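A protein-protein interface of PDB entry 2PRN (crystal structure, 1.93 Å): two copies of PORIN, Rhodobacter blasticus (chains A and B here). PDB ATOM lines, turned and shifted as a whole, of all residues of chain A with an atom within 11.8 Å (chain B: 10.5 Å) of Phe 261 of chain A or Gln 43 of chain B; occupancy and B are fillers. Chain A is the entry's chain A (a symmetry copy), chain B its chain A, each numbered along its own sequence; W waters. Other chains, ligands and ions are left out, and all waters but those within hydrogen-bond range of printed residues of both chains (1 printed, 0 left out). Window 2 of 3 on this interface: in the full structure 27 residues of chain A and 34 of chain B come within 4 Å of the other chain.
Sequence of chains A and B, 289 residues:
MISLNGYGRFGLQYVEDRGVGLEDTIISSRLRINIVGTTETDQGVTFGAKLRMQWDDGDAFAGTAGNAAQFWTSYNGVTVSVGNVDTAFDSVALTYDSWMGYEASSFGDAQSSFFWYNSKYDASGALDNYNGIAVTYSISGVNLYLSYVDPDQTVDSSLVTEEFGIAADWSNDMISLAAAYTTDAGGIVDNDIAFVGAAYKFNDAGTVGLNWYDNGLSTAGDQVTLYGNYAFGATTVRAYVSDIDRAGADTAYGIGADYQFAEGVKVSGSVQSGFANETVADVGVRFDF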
ATOM      1  N   PHE A  10     -17.040  -8.266  35.401  1.00  0.00           N
ATOM      2  CA  PHE A  10     -15.656  -8.426  35.868  1.00  0.00           C
ATOM      3  C   PHE A  10     -14.750  -8.787  34.686  1.00  0.00           C
ATOM      4  O   PHE A  10     -15.187  -9.456  33.725  1.00  0.00           O
ATOM      5  CB  PHE A  10     -15.552  -9.447  37.015  1.00  0.00           C
ATOM      6  CG  PHE A  10     -15.904 -10.876  36.705  1.00  0.00           C
ATOM      7  CD1 PHE A  10     -14.979 -11.735  36.127  1.00  0.00           C
ATOM      8  CD2 PHE A  10     -17.168 -11.377  36.950  1.00  0.00           C
ATOM      9  CE1 PHE A  10     -15.291 -13.047  35.844  1.00  0.00           C
ATOM     10  CE2 PHE A  10     -17.477 -12.698  36.683  1.00  0.00           C
ATOM     11  CZ  PHE A  10     -16.548 -13.541  36.128  1.00  0.00           C
ATOM     12  N   PHE A 232     -22.078 -10.753  13.214  1.00  0.00           N
ATOM     13  CA  PHE A 232     -21.823 -12.018  12.554  1.00  0.00           C
ATOM     14  C   PHE A 232     -22.438 -13.118  13.434  1.00  0.00           C
ATOM     15  O   PHE A 232     -21.729 -13.833  14.140  1.00  0.00           O
ATOM     16  CB  PHE A 232     -20.329 -12.303  12.461  1.00  0.00           C
ATOM     17  CG  PHE A 232     -19.517 -11.379  11.625  1.00  0.00           C
ATOM     18  CD1 PHE A 232     -19.588 -11.439  10.228  1.00  0.00           C
ATOM     19  CD2 PHE A 232     -18.627 -10.481  12.204  1.00  0.00           C
ATOM     20  CE1 PHE A 232     -18.813 -10.611   9.436  1.00  0.00           C
ATOM     21  CE2 PHE A 232     -17.857  -9.640  11.411  1.00  0.00           C
ATOM     22  CZ  PHE A 232     -17.951  -9.707  10.023  1.00  0.00           C
ATOM     23  N   GLY A 233     -23.766 -13.223  13.424  1.00  0.00           N
ATOM     24  CA  GLY A 233     -24.326 -14.293  14.299  1.00  0.00           C
ATOM     25  C   GLY A 233     -24.273 -13.814  15.753  1.00  0.00           C
ATOM     26  O   GLY A 233     -24.930 -12.813  16.048  1.00  0.00           O
ATOM     27  N   ALA A 234     -23.545 -14.496  16.629  1.00  0.00           N
ATOM     28  CA  ALA A 234     -23.541 -14.039  18.033  1.00  0.00           C
ATOM     29  C   ALA A 234     -22.425 -13.043  18.293  1.00  0.00           C
ATOM     30  O   ALA A 234     -22.314 -12.462  19.377  1.00  0.00           O
ATOM     31  CB  ALA A 234     -23.439 -15.197  19.001  1.00  0.00           C
ATOM     32  N   THR A 235     -21.525 -12.902  17.296  1.00  0.00           N
ATOM     33  CA  THR A 235     -20.412 -12.007  17.555  1.00  0.00           C
ATOM     34  C   THR A 235     -20.550 -10.683  16.842  1.00  0.00           C
ATOM     35  O   THR A 235     -20.875 -10.601  15.655  1.00  0.00           O
ATOM     36  CB  THR A 235     -19.053 -12.674  17.472  1.00  0.00           C
ATOM     37  OG1 THR A 235     -18.188 -11.905  16.637  1.00  0.00           O
ATOM     38  CG2 THR A 235     -19.093 -14.109  16.986  1.00  0.00           C
ATOM     39  N   THR A 236     -20.379  -9.593  17.599  1.00  0.00           N
ATOM     40  CA  THR A 236     -20.457  -8.241  17.079  1.00  0.00           C
ATOM     41  C   THR A 236     -19.065  -7.600  17.057  1.00  0.00           C
ATOM     42  O   THR A 236     -18.310  -7.619  18.026  1.00  0.00           O
ATOM     43  CB  THR A 236     -21.433  -7.346  17.822  1.00  0.00           C
ATOM     44  OG1 THR A 236     -22.722  -7.957  17.833  1.00  0.00           O
ATOM     45  CG2 THR A 236     -21.582  -5.959  17.191  1.00  0.00           C
ATOM     46  N   ALA A 257     -14.880  -6.329  20.169  1.00  0.00           N
ATOM     47  CA  ALA A 257     -15.859  -7.362  19.834  1.00  0.00           C
ATOM     48  C   ALA A 257     -16.701  -7.750  21.058  1.00  0.00           C
ATOM     49  O   ALA A 257     -16.282  -7.660  22.209  1.00  0.00           O
ATOM     50  CB  ALA A 257     -15.126  -8.580  19.301  1.00  0.00           C
ATOM     51  N   ASP A 258     -17.929  -8.114  20.757  1.00  0.00           N
ATOM     52  CA  ASP A 258     -18.847  -8.653  21.725  1.00  0.00           C
ATOM     53  C   ASP A 258     -19.283 -10.050  21.256  1.00  0.00           C
ATOM     54  O   ASP A 258     -19.483 -10.304  20.060  1.00  0.00           O
ATOM     55  CB  ASP A 258     -20.097  -7.829  21.915  1.00  0.00           C
ATOM     56  CG  ASP A 258     -19.863  -6.381  22.257  1.00  0.00           C
ATOM     57  OD1 ASP A 258     -18.933  -6.062  23.030  1.00  0.00           O
ATOM     58  OD2 ASP A 258     -20.627  -5.542  21.751  1.00  0.00           O
ATOM     59  N   TYR A 259     -19.453 -10.897  22.249  1.00  0.00           N
ATOM     60  CA  TYR A 259     -19.942 -12.246  21.995  1.00  0.00           C
ATOM     61  C   TYR A 259     -21.121 -12.494  22.948  1.00  0.00           C
ATOM     62  O   TYR A 259     -20.969 -12.389  24.174  1.00  0.00           O
ATOM     63  CB  TYR A 259     -18.815 -13.251  22.164  1.00  0.00           C
ATOM     64  CG  TYR A 259     -19.325 -14.673  21.996  1.00  0.00           C
ATOM     65  CD1 TYR A 259     -19.665 -15.071  20.701  1.00  0.00           C
ATOM     66  CD2 TYR A 259     -19.474 -15.560  23.035  1.00  0.00           C
ATOM     67  CE1 TYR A 259     -20.147 -16.344  20.458  1.00  0.00           C
ATOM     68  CE2 TYR A 259     -19.966 -16.840  22.805  1.00  0.00           C
ATOM     69  CZ  TYR A 259     -20.279 -17.213  21.518  1.00  0.00           C
ATOM     70  OH  TYR A 259     -20.770 -18.475  21.237  1.00  0.00           O
ATOM     71  N   GLN A 260     -22.277 -12.714  22.357  1.00  0.00           N
ATOM     72  CA  GLN A 260     -23.489 -12.978  23.166  1.00  0.00           C
ATOM     73  C   GLN A 260     -23.494 -14.443  23.566  1.00  0.00           C
ATOM     74  O   GLN A 260     -23.975 -15.327  22.859  1.00  0.00           O
ATOM     75  CB  GLN A 260     -24.749 -12.629  22.400  1.00  0.00           C
ATOM     76  CG  GLN A 260     -25.950 -12.351  23.288  1.00  0.00           C
ATOM     77  CD  GLN A 260     -25.924 -11.096  24.116  1.00  0.00           C
ATOM     78  OE1 GLN A 260     -25.428 -10.021  23.699  1.00  0.00           O
ATOM     79  NE2 GLN A 260     -26.466 -11.145  25.343  1.00  0.00           N
ATOM     80  N   PHE A 261     -22.924 -14.720  24.721  1.00  0.00           N
ATOM     81  CA  PHE A 261     -22.841 -16.110  25.182  1.00  0.00           C
ATOM     82  C   PHE A 261     -24.208 -16.734  25.455  1.00  0.00           C
ATOM     83  O   PHE A 261     -24.403 -17.939  25.249  1.00  0.00           O
ATOM     84  CB  PHE A 261     -21.949 -16.084  26.417  1.00  0.00           C
ATOM     85  CG  PHE A 261     -21.819 -17.419  27.085  1.00  0.00           C
ATOM     86  CD1 PHE A 261     -21.025 -18.405  26.503  1.00  0.00           C
ATOM     87  CD2 PHE A 261     -22.492 -17.714  28.249  1.00  0.00           C
ATOM     88  CE1 PHE A 261     -20.889 -19.641  27.121  1.00  0.00           C
ATOM     89  CE2 PHE A 261     -22.361 -18.931  28.865  1.00  0.00           C
ATOM     90  CZ  PHE A 261     -21.542 -19.903  28.298  1.00  0.00           C
ATOM     91  N   ALA A 262     -25.139 -15.959  25.922  1.00  0.00           N
ATOM     92  CA  ALA A 262     -26.470 -16.364  26.324  1.00  0.00           C
ATOM     93  C   ALA A 262     -27.286 -15.112  26.549  1.00  0.00           C
ATOM     94  O   ALA A 262     -26.726 -14.007  26.477  1.00  0.00           O
ATOM     95  CB  ALA A 262     -26.431 -17.279  27.548  1.00  0.00           C
ATOM     96  N   GLU A 263     -28.576 -15.209  26.717  1.00  0.00           N
ATOM     97  CA  GLU A 263     -29.451 -14.085  26.982  1.00  0.00           C
ATOM     98  C   GLU A 263     -28.935 -13.481  28.301  1.00  0.00           C
ATOM     99  O   GLU A 263     -28.732 -14.273  29.258  1.00  0.00           O
ATOM    100  CB  GLU A 263     -30.884 -14.621  27.183  1.00  0.00           C
ATOM    101  CG  GLU A 263     -31.911 -13.502  27.169  1.00  0.00           C
ATOM    102  CD  GLU A 263     -33.320 -13.930  27.534  1.00  0.00           C
ATOM    103  OE1 GLU A 263     -33.812 -14.996  27.064  1.00  0.00           O
ATOM    104  OE2 GLU A 263     -33.999 -13.168  28.290  1.00  0.00           O
ATOM    105  N   GLY A 264     -28.699 -12.196  28.362  1.00  0.00           N
ATOM    106  CA  GLY A 264     -28.188 -11.607  29.580  1.00  0.00           C
ATOM    107  C   GLY A 264     -26.716 -11.836  29.850  1.00  0.00           C
ATOM    108  O   GLY A 264     -26.263 -11.329  30.911  1.00  0.00           O
ATOM    109  N   VAL A 265     -25.932 -12.540  29.021  1.00  0.00           N
ATOM    110  CA  VAL A 265     -24.506 -12.724  29.310  1.00  0.00           C
ATOM    111  C   VAL A 265     -23.668 -12.258  28.098  1.00  0.00           C
ATOM    112  O   VAL A 265     -23.816 -12.836  27.006  1.00  0.00           O
ATOM    113  CB  VAL A 265     -24.089 -14.139  29.687  1.00  0.00           C
ATOM    114  CG1 VAL A 265     -22.595 -14.271  29.982  1.00  0.00           C
ATOM    115  CG2 VAL A 265     -24.881 -14.656  30.894  1.00  0.00           C
ATOM    116  N   LYS A 266     -22.849 -11.235  28.300  1.00  0.00           N
ATOM    117  CA  LYS A 266     -22.061 -10.710  27.151  1.00  0.00           C
ATOM    118  C   LYS A 266     -20.584 -10.696  27.442  1.00  0.00           C
ATOM    119  O   LYS A 266     -20.145 -10.174  28.480  1.00  0.00           O
ATOM    120  CB  LYS A 266     -22.604  -9.313  26.839  1.00  0.00           C
ATOM    121  CG  LYS A 266     -21.981  -8.644  25.628  1.00  0.00           C
ATOM    122  CD  LYS A 266     -23.053  -7.754  24.985  1.00  0.00           C
ATOM    123  CE  LYS A 266     -22.872  -6.315  25.455  1.00  0.00           C
ATOM    124  NZ  LYS A 266     -24.130  -5.550  25.072  1.00  0.00           N
ATOM    125  N   VAL A 267     -19.771 -11.330  26.581  1.00  0.00           N
ATOM    126  CA  VAL A 267     -18.312 -11.294  26.772  1.00  0.00           C
ATOM    127  C   VAL A 267     -17.771 -10.198  25.861  1.00  0.00           C
ATOM    128  O   VAL A 267     -18.226 -10.186  24.708  1.00  0.00           O
ATOM    129  CB  VAL A 267     -17.671 -12.626  26.392  1.00  0.00           C
ATOM    130  CG1 VAL A 267     -16.182 -12.629  26.764  1.00  0.00           C
ATOM    131  CG2 VAL A 267     -18.377 -13.722  27.219  1.00  0.00           C
ATOM    132  N   SER A 268     -16.975  -9.247  26.333  1.00  0.00           N
ATOM    133  CA  SER A 268     -16.550  -8.158  25.486  1.00  0.00           C
ATOM    134  C   SER A 268     -15.074  -7.830  25.718  1.00  0.00           C
ATOM    135  O   SER A 268     -14.610  -7.991  26.836  1.00  0.00           O
ATOM    136  CB  SER A 268     -17.279  -6.843  25.716  1.00  0.00           C
ATOM    137  OG  SER A 268     -18.659  -6.976  25.587  1.00  0.00           O
ATOM    138  N   GLY A 269     -14.474  -7.235  24.694  1.00  0.00           N
ATOM    139  CA  GLY A 269     -13.071  -6.843  24.751  1.00  0.00           C
ATOM    140  C   GLY A 269     -12.829  -5.658  23.799  1.00  0.00           C
ATOM    141  O   GLY A 269     -13.582  -5.405  22.888  1.00  0.00           O
ATOM    142  N   GLY A 284     -13.621  -8.873  29.391  1.00  0.00           N
ATOM    143  CA  GLY A 284     -14.429  -9.320  30.521  1.00  0.00           C
ATOM    144  C   GLY A 284     -15.845  -9.720  30.152  1.00  0.00           C
ATOM    145  O   GLY A 284     -16.229  -9.753  28.982  1.00  0.00           O
ATOM    146  N   VAL A 285     -16.601 -10.031  31.203  1.00  0.00           N
ATOM    147  CA  VAL A 285     -17.985 -10.429  31.084  1.00  0.00           C
ATOM    148  C   VAL A 285     -18.924  -9.494  31.859  1.00  0.00           C
ATOM    149  O   VAL A 285     -18.600  -9.061  32.965  1.00  0.00           O
ATOM    150  CB  VAL A 285     -18.348 -11.767  31.767  1.00  0.00           C
ATOM    151  CG1 VAL A 285     -19.062 -12.707  30.816  1.00  0.00           C
ATOM    152  CG2 VAL A 285     -17.164 -12.481  32.390  1.00  0.00           C
ATOM    153  N   ARG A 286     -20.086  -9.314  31.289  1.00  0.00           N
ATOM    154  CA  ARG A 286     -21.182  -8.627  31.949  1.00  0.00           C
ATOM    155  C   ARG A 286     -22.378  -9.627  31.972  1.00  0.00           C
ATOM    156  O   ARG A 286     -22.725 -10.217  30.927  1.00  0.00           O
ATOM    157  CB  ARG A 286     -21.607  -7.341  31.245  1.00  0.00           C
ATOM    158  CG  ARG A 286     -22.849  -6.719  31.891  1.00  0.00           C
ATOM    159  CD  ARG A 286     -23.419  -5.543  31.114  1.00  0.00           C
ATOM    160  NE  ARG A 286     -24.820  -5.281  31.448  1.00  0.00           N
ATOM    161  CZ  ARG A 286     -25.368  -4.074  31.533  1.00  0.00           C
ATOM    162  NH1 ARG A 286     -24.620  -2.987  31.312  1.00  0.00           N
ATOM    163  NH2 ARG A 286     -26.650  -3.875  31.819  1.00  0.00           N
ATOM    164  N   PHE A 287     -23.009  -9.766  33.107  1.00  0.00           N
ATOM    165  CA  PHE A 287     -24.192 -10.574  33.266  1.00  0.00           C
ATOM    166  C   PHE A 287     -25.285  -9.797  33.992  1.00  0.00           C
ATOM    167  O   PHE A 287     -25.082  -9.117  35.017  1.00  0.00           O
ATOM    168  CB  PHE A 287     -23.859 -11.928  33.903  1.00  0.00           C
ATOM    169  CG  PHE A 287     -23.167 -11.821  35.237  1.00  0.00           C
ATOM    170  CD1 PHE A 287     -21.809 -11.624  35.331  1.00  0.00           C
ATOM    171  CD2 PHE A 287     -23.918 -11.878  36.410  1.00  0.00           C
ATOM    172  CE1 PHE A 287     -21.166 -11.560  36.558  1.00  0.00           C
ATOM    173  CE2 PHE A 287     -23.311 -11.822  37.646  1.00  0.00           C
ATOM    174  CZ  PHE A 287     -21.924 -11.699  37.714  1.00  0.00           C
ATOM    175  N   ASP A 288     -26.474  -9.768  33.387  1.00  0.00           N
ATOM    176  CA  ASP A 288     -27.632  -9.065  33.855  1.00  0.00           C
ATOM    177  C   ASP A 288     -28.559  -9.966  34.671  1.00  0.00           C
ATOM    178  O   ASP A 288     -28.670 -11.123  34.300  1.00  0.00           O
ATOM    179  CB  ASP A 288     -28.454  -8.495  32.670  1.00  0.00           C
ATOM    180  CG  ASP A 288     -27.704  -7.290  32.118  1.00  0.00           C
ATOM    181  OD1 ASP A 288     -26.616  -7.462  31.502  1.00  0.00           O
ATOM    182  OD2 ASP A 288     -28.156  -6.137  32.340  1.00  0.00           O
ATOM    183  N   THR B  39     -27.505 -15.295  37.152  1.00  0.00           N
ATOM    184  CA  THR B  39     -27.865 -15.373  35.746  1.00  0.00           C
ATOM    185  C   THR B  39     -27.582 -16.847  35.342  1.00  0.00           C
ATOM    186  O   THR B  39     -26.417 -17.261  35.315  1.00  0.00           O
ATOM    187  CB  THR B  39     -27.033 -14.401  34.888  1.00  0.00           C
ATOM    188  OG1 THR B  39     -27.142 -13.045  35.406  1.00  0.00           O
ATOM    189  CG2 THR B  39     -27.508 -14.392  33.447  1.00  0.00           C
ATOM    190  N   GLU B  40     -28.610 -17.603  35.118  1.00  0.00           N
ATOM    191  CA  GLU B  40     -28.521 -19.016  34.701  1.00  0.00           C
ATOM    192  C   GLU B  40     -28.476 -19.053  33.195  1.00  0.00           C
ATOM    193  O   GLU B  40     -29.029 -18.148  32.526  1.00  0.00           O
ATOM    194  CB  GLU B  40     -29.763 -19.777  35.215  1.00  0.00           C
ATOM    195  CG  GLU B  40     -29.695 -19.867  36.742  1.00  0.00           C
ATOM    196  CD  GLU B  40     -30.906 -20.546  37.373  1.00  0.00           C
ATOM    197  OE1 GLU B  40     -31.875 -20.914  36.658  1.00  0.00           O
ATOM    198  OE2 GLU B  40     -30.893 -20.716  38.640  1.00  0.00           O
ATOM    199  N   THR B  41     -27.707 -19.935  32.573  1.00  0.00           N
ATOM    200  CA  THR B  41     -27.647 -19.990  31.119  1.00  0.00           C
ATOM    201  C   THR B  41     -28.036 -21.423  30.694  1.00  0.00           C
ATOM    202  O   THR B  41     -27.920 -22.370  31.455  1.00  0.00           O
ATOM    203  CB  THR B  41     -26.278 -19.677  30.482  1.00  0.00           C
ATOM    204  OG1 THR B  41     -25.328 -20.659  30.935  1.00  0.00           O
ATOM    205  CG2 THR B  41     -25.758 -18.313  30.908  1.00  0.00           C
ATOM    206  N   ASP B  42     -28.407 -21.549  29.418  1.00  0.00           N
ATOM    207  CA  ASP B  42     -28.790 -22.887  28.960  1.00  0.00           C
ATOM    208  C   ASP B  42     -27.561 -23.730  28.681  1.00  0.00           C
ATOM    209  O   ASP B  42     -27.703 -24.924  28.449  1.00  0.00           O
ATOM    210  CB  ASP B  42     -29.751 -22.840  27.801  1.00  0.00           C
ATOM    211  CG  ASP B  42     -29.276 -22.170  26.535  1.00  0.00           C
ATOM    212  OD1 ASP B  42     -28.050 -21.912  26.350  1.00  0.00           O
ATOM    213  OD2 ASP B  42     -30.148 -21.867  25.659  1.00  0.00           O
ATOM    214  N   GLN B  43     -26.381 -23.127  28.708  1.00  0.00           N
ATOM    215  CA  GLN B  43     -25.142 -23.852  28.487  1.00  0.00           C
ATOM    216  C   GLN B  43     -24.743 -24.508  29.801  1.00  0.00           C
ATOM    217  O   GLN B  43     -23.774 -25.265  29.858  1.00  0.00           O
ATOM    218  CB  GLN B  43     -24.050 -22.896  27.988  1.00  0.00           C
ATOM    219  CG  GLN B  43     -24.558 -21.963  26.884  1.00  0.00           C
ATOM    220  CD  GLN B  43     -24.736 -22.744  25.593  1.00  0.00           C
ATOM    221  OE1 GLN B  43     -23.861 -23.546  25.254  1.00  0.00           O
ATOM    222  NE2 GLN B  43     -25.821 -22.561  24.855  1.00  0.00           N
ATOM    223  N   GLY B  44     -25.439 -24.202  30.903  1.00  0.00           N
ATOM    224  CA  GLY B  44     -25.085 -24.824  32.185  1.00  0.00           C
ATOM    225  C   GLY B  44     -24.063 -24.044  33.002  1.00  0.00           C
ATOM    226  O   GLY B  44     -23.478 -24.543  33.991  1.00  0.00           O
ATOM    227  N   VAL B  45     -23.738 -22.832  32.609  1.00  0.00           N
ATOM    228  CA  VAL B  45     -22.867 -21.926  33.294  1.00  0.00           C
ATOM    229  C   VAL B  45     -23.718 -20.917  34.068  1.00  0.00           C
ATOM    230  O   VAL B  45     -24.619 -20.348  33.458  1.00  0.00           O
ATOM    231  CB  VAL B  45     -21.943 -21.140  32.338  1.00  0.00           C
ATOM    232  CG1 VAL B  45     -20.952 -20.336  33.195  1.00  0.00           C
ATOM    233  CG2 VAL B  45     -21.190 -22.140  31.461  1.00  0.00           C
ATOM    234  N   THR B  46     -23.477 -20.777  35.343  1.00  0.00           N
ATOM    235  CA  THR B  46     -24.208 -19.818  36.165  1.00  0.00           C
ATOM    236  C   THR B  46     -23.247 -18.689  36.534  1.00  0.00           C
ATOM    237  O   THR B  46     -22.083 -18.928  36.871  1.00  0.00           O
ATOM    238  CB  THR B  46     -24.686 -20.517  37.471  1.00  0.00           C
ATOM    239  OG1 THR B  46     -25.611 -21.527  37.111  1.00  0.00           O
ATOM    240  CG2 THR B  46     -25.417 -19.528  38.366  1.00  0.00           C
ATOM    241  N   PHE B  47     -23.695 -17.470  36.465  1.00  0.00           N
ATOM    242  CA  PHE B  47     -22.980 -16.277  36.882  1.00  0.00           C
ATOM    243  C   PHE B  47     -23.713 -15.739  38.105  1.00  0.00           C
ATOM    244  O   PHE B  47     -24.945 -15.764  38.162  1.00  0.00           O
ATOM    245  CB  PHE B  47     -22.859 -15.198  35.789  1.00  0.00           C
ATOM    246  CG  PHE B  47     -22.125 -15.701  34.577  1.00  0.00           C
ATOM    247  CD1 PHE B  47     -22.774 -16.478  33.623  1.00  0.00           C
ATOM    248  CD2 PHE B  47     -20.774 -15.400  34.396  1.00  0.00           C
ATOM    249  CE1 PHE B  47     -22.082 -16.945  32.505  1.00  0.00           C
ATOM    250  CE2 PHE B  47     -20.116 -15.857  33.270  1.00  0.00           C
ATOM    251  CZ  PHE B  47     -20.753 -16.652  32.329  1.00  0.00           C
ATOM    252  N   THR B  73     -18.502 -17.609  38.832  1.00  0.00           N
ATOM    253  CA  THR B  73     -18.898 -18.320  37.634  1.00  0.00           C
ATOM    254  C   THR B  73     -18.815 -19.823  37.989  1.00  0.00           C
ATOM    255  O   THR B  73     -17.791 -20.264  38.531  1.00  0.00           O
ATOM    256  CB  THR B  73     -18.010 -18.084  36.422  1.00  0.00           C
ATOM    257  OG1 THR B  73     -17.908 -16.676  36.147  1.00  0.00           O
ATOM    258  CG2 THR B  73     -18.657 -18.740  35.212  1.00  0.00           C
ATOM    259  N   SER B  74     -19.892 -20.534  37.750  1.00  0.00           N
ATOM    260  CA  SER B  74     -20.003 -21.936  38.102  1.00  0.00           C
ATOM    261  C   SER B  74     -20.321 -22.841  36.918  1.00  0.00           C
ATOM    262  O   SER B  74     -21.263 -22.539  36.183  1.00  0.00           O
ATOM    263  CB  SER B  74     -21.190 -22.174  39.053  1.00  0.00           C
ATOM    264  OG  SER B  74     -20.694 -22.270  40.365  1.00  0.00           O
ATOM    265  N   TYR B  75     -19.635 -23.976  36.855  1.00  0.00           N
ATOM    266  CA  TYR B  75     -19.862 -24.921  35.765  1.00  0.00           C
ATOM    267  C   TYR B  75     -19.340 -26.308  36.116  1.00  0.00           C
ATOM    268  O   TYR B  75     -18.159 -26.447  36.382  1.00  0.00           O
ATOM    269  CB  TYR B  75     -19.090 -24.440  34.530  1.00  0.00           C
ATOM    270  CG  TYR B  75     -19.242 -25.368  33.342  1.00  0.00           C
ATOM    271  CD1 TYR B  75     -20.483 -25.586  32.759  1.00  0.00           C
ATOM    272  CD2 TYR B  75     -18.130 -26.012  32.815  1.00  0.00           C
ATOM    273  CE1 TYR B  75     -20.610 -26.433  31.681  1.00  0.00           C
ATOM    274  CE2 TYR B  75     -18.241 -26.867  31.728  1.00  0.00           C
ATOM    275  CZ  TYR B  75     -19.495 -27.071  31.172  1.00  0.00           C
ATOM    276  OH  TYR B  75     -19.618 -27.914  30.097  1.00  0.00           O
ATOM    277  N   ASN B  76     -20.231 -27.275  36.128  1.00  0.00           N
ATOM    278  CA  ASN B  76     -19.865 -28.664  36.361  1.00  0.00           C
ATOM    279  C   ASN B  76     -19.075 -28.905  37.628  1.00  0.00           C
ATOM    280  O   ASN B  76     -18.008 -29.554  37.550  1.00  0.00           O
ATOM    281  CB  ASN B  76     -18.951 -29.035  35.157  1.00  0.00           C
ATOM    282  CG  ASN B  76     -19.636 -30.024  34.246  1.00  0.00           C
ATOM    283  OD1 ASN B  76     -20.294 -29.626  33.275  1.00  0.00           O
ATOM    284  ND2 ASN B  76     -19.468 -31.306  34.603  1.00  0.00           N
ATOM    285  N   GLY B  77     -19.554 -28.406  38.757  1.00  0.00           N
ATOM    286  CA  GLY B  77     -18.852 -28.628  40.025  1.00  0.00           C
ATOM    287  C   GLY B  77     -17.680 -27.703  40.248  1.00  0.00           C
ATOM    288  O   GLY B  77     -17.045 -27.747  41.332  1.00  0.00           O
HETATM  289  O   HOH W   1     -29.556 -17.121  29.958  1.00  0.00           O
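OG1 of Thr 73 of chain B touches CZ of Phe 10 of chain A, 3.4 Å away.
CZ of Phe 261 of chain A touches CG of Gln 43 of chain B, at 3.9 Å.
Val 45 of chain B touches Phe 261 of chain A.
Ala 262 of chain A touches Thr 41 of chain B.
Val 265 of chain A touches Thr 39 of chain B.
Val 265 of chain A touches Thr 41 of chain B (CG2 to CG2, 3.8 Å).
CE1 of Phe 47 of chain B touches CG1 of Val 265 of chain A (3.7 Å).
OG1 of Thr 39 of chain B touches CD2 of Phe 287 of chain A, at 3.6 Å.
CG of Phe 287 of chain A touches CB of Phe 47 of chain B, at 3.4 Å.
Of the 14 printed residues of chain B, 6 touch a printed residue of chain A.
Hydrophobic or aromatic side chains of chain B that line the printed part of chain A: Val 45 and Phe 47.
Along chain B the printed residues that touch a printed residue of chain A span positions 39 to 73.
Among the printed residues, 10 pairs touch across the chains.
O of Phe 47 of chain B lies within hydrogen-bond range of N of Thr 39 of chain B, 2.8 Å away.
The backbone NH of Gln 43 of chain B sits close to the side-chain hydroxyl of Thr 41 of chain B.
The side-chain hydroxyl (OG1) of Thr 41 of chain B sits at hydrogen-bond distance from the backbone carbonyl oxygen (O) of Val 45 of chain B (2.6 Å).
The side-chain carboxylate (OD1) of Asp 42 of chain B lies within hydrogen-bond range of the side-chain amide nitrogen (NE2) of Gln 43 of chain B (2.8 Å).
The backbone NH of Val 285 of chain A is in hydrogen-bond range of the backbone carbonyl oxygen of Phe 10 of chain A (2.9 Å).
OD2 of Asp 288 of chain A lies within salt-bridge range of NH2 of Arg 286 of chain A.
Water W1 bridges O of Glu 40 of chain B (2.8 Å) and O of Glu 263 of chain A (3.0 Å).
The side-chain hydroxyl (OG1) of Thr 39 of chain B sits at hydrogen-bond distance from the backbone carbonyl oxygen (O) of Asp 288 of chain A, 2.7 Å away.
No position is printed for both chains.
Of the printed residues of chain B, Phe 261 of chain A touches Gln 43 and Val 45.
Gln 43 of chain B touches one residue of chain A.
No residue of chain B comes within 4 Å of Tyr 259 of chain A.
Of the printed residues of chain B, Ala 262 of chain A touches Thr 41 (3.6 Å).
Val 265 of chain A touches just these residues of chain B: Thr 39 (3.7 Å), Thr 41 (3.8 Å) and Phe 47 (3.7 Å).
No residue of chain A comes within 4 Å of Gly 44 of chain B.
Val 45 of chain B touches just one residue of chain A: Phe 261.
Of the printed residues of chain B, Phe 10 of chain A touches Thr 73.
Of the printed residues of chain A, Thr 39 of chain B touches Val 265, Phe 287 and Asp 288.
Of the printed residues of chain A, Phe 47 of chain B touches Val 265 (3.7 Å) and Phe 287 (3.4 Å).
Printed residues of chain A within 4 Å of Thr 41 of chain B: Ala 262 and Val 265.
Printed residues of chain A within 4 Å of Thr 73 of chain B: Phe 10.
Gly 284 of chain A touches none of the printed residues of chain B.
Tyr 75 of chain B touches none of the printed residues of chain A.
The nearest residue of chain A that does not touch Gln 43 of chain B is Ala 262 of chain A (5.1 Å).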
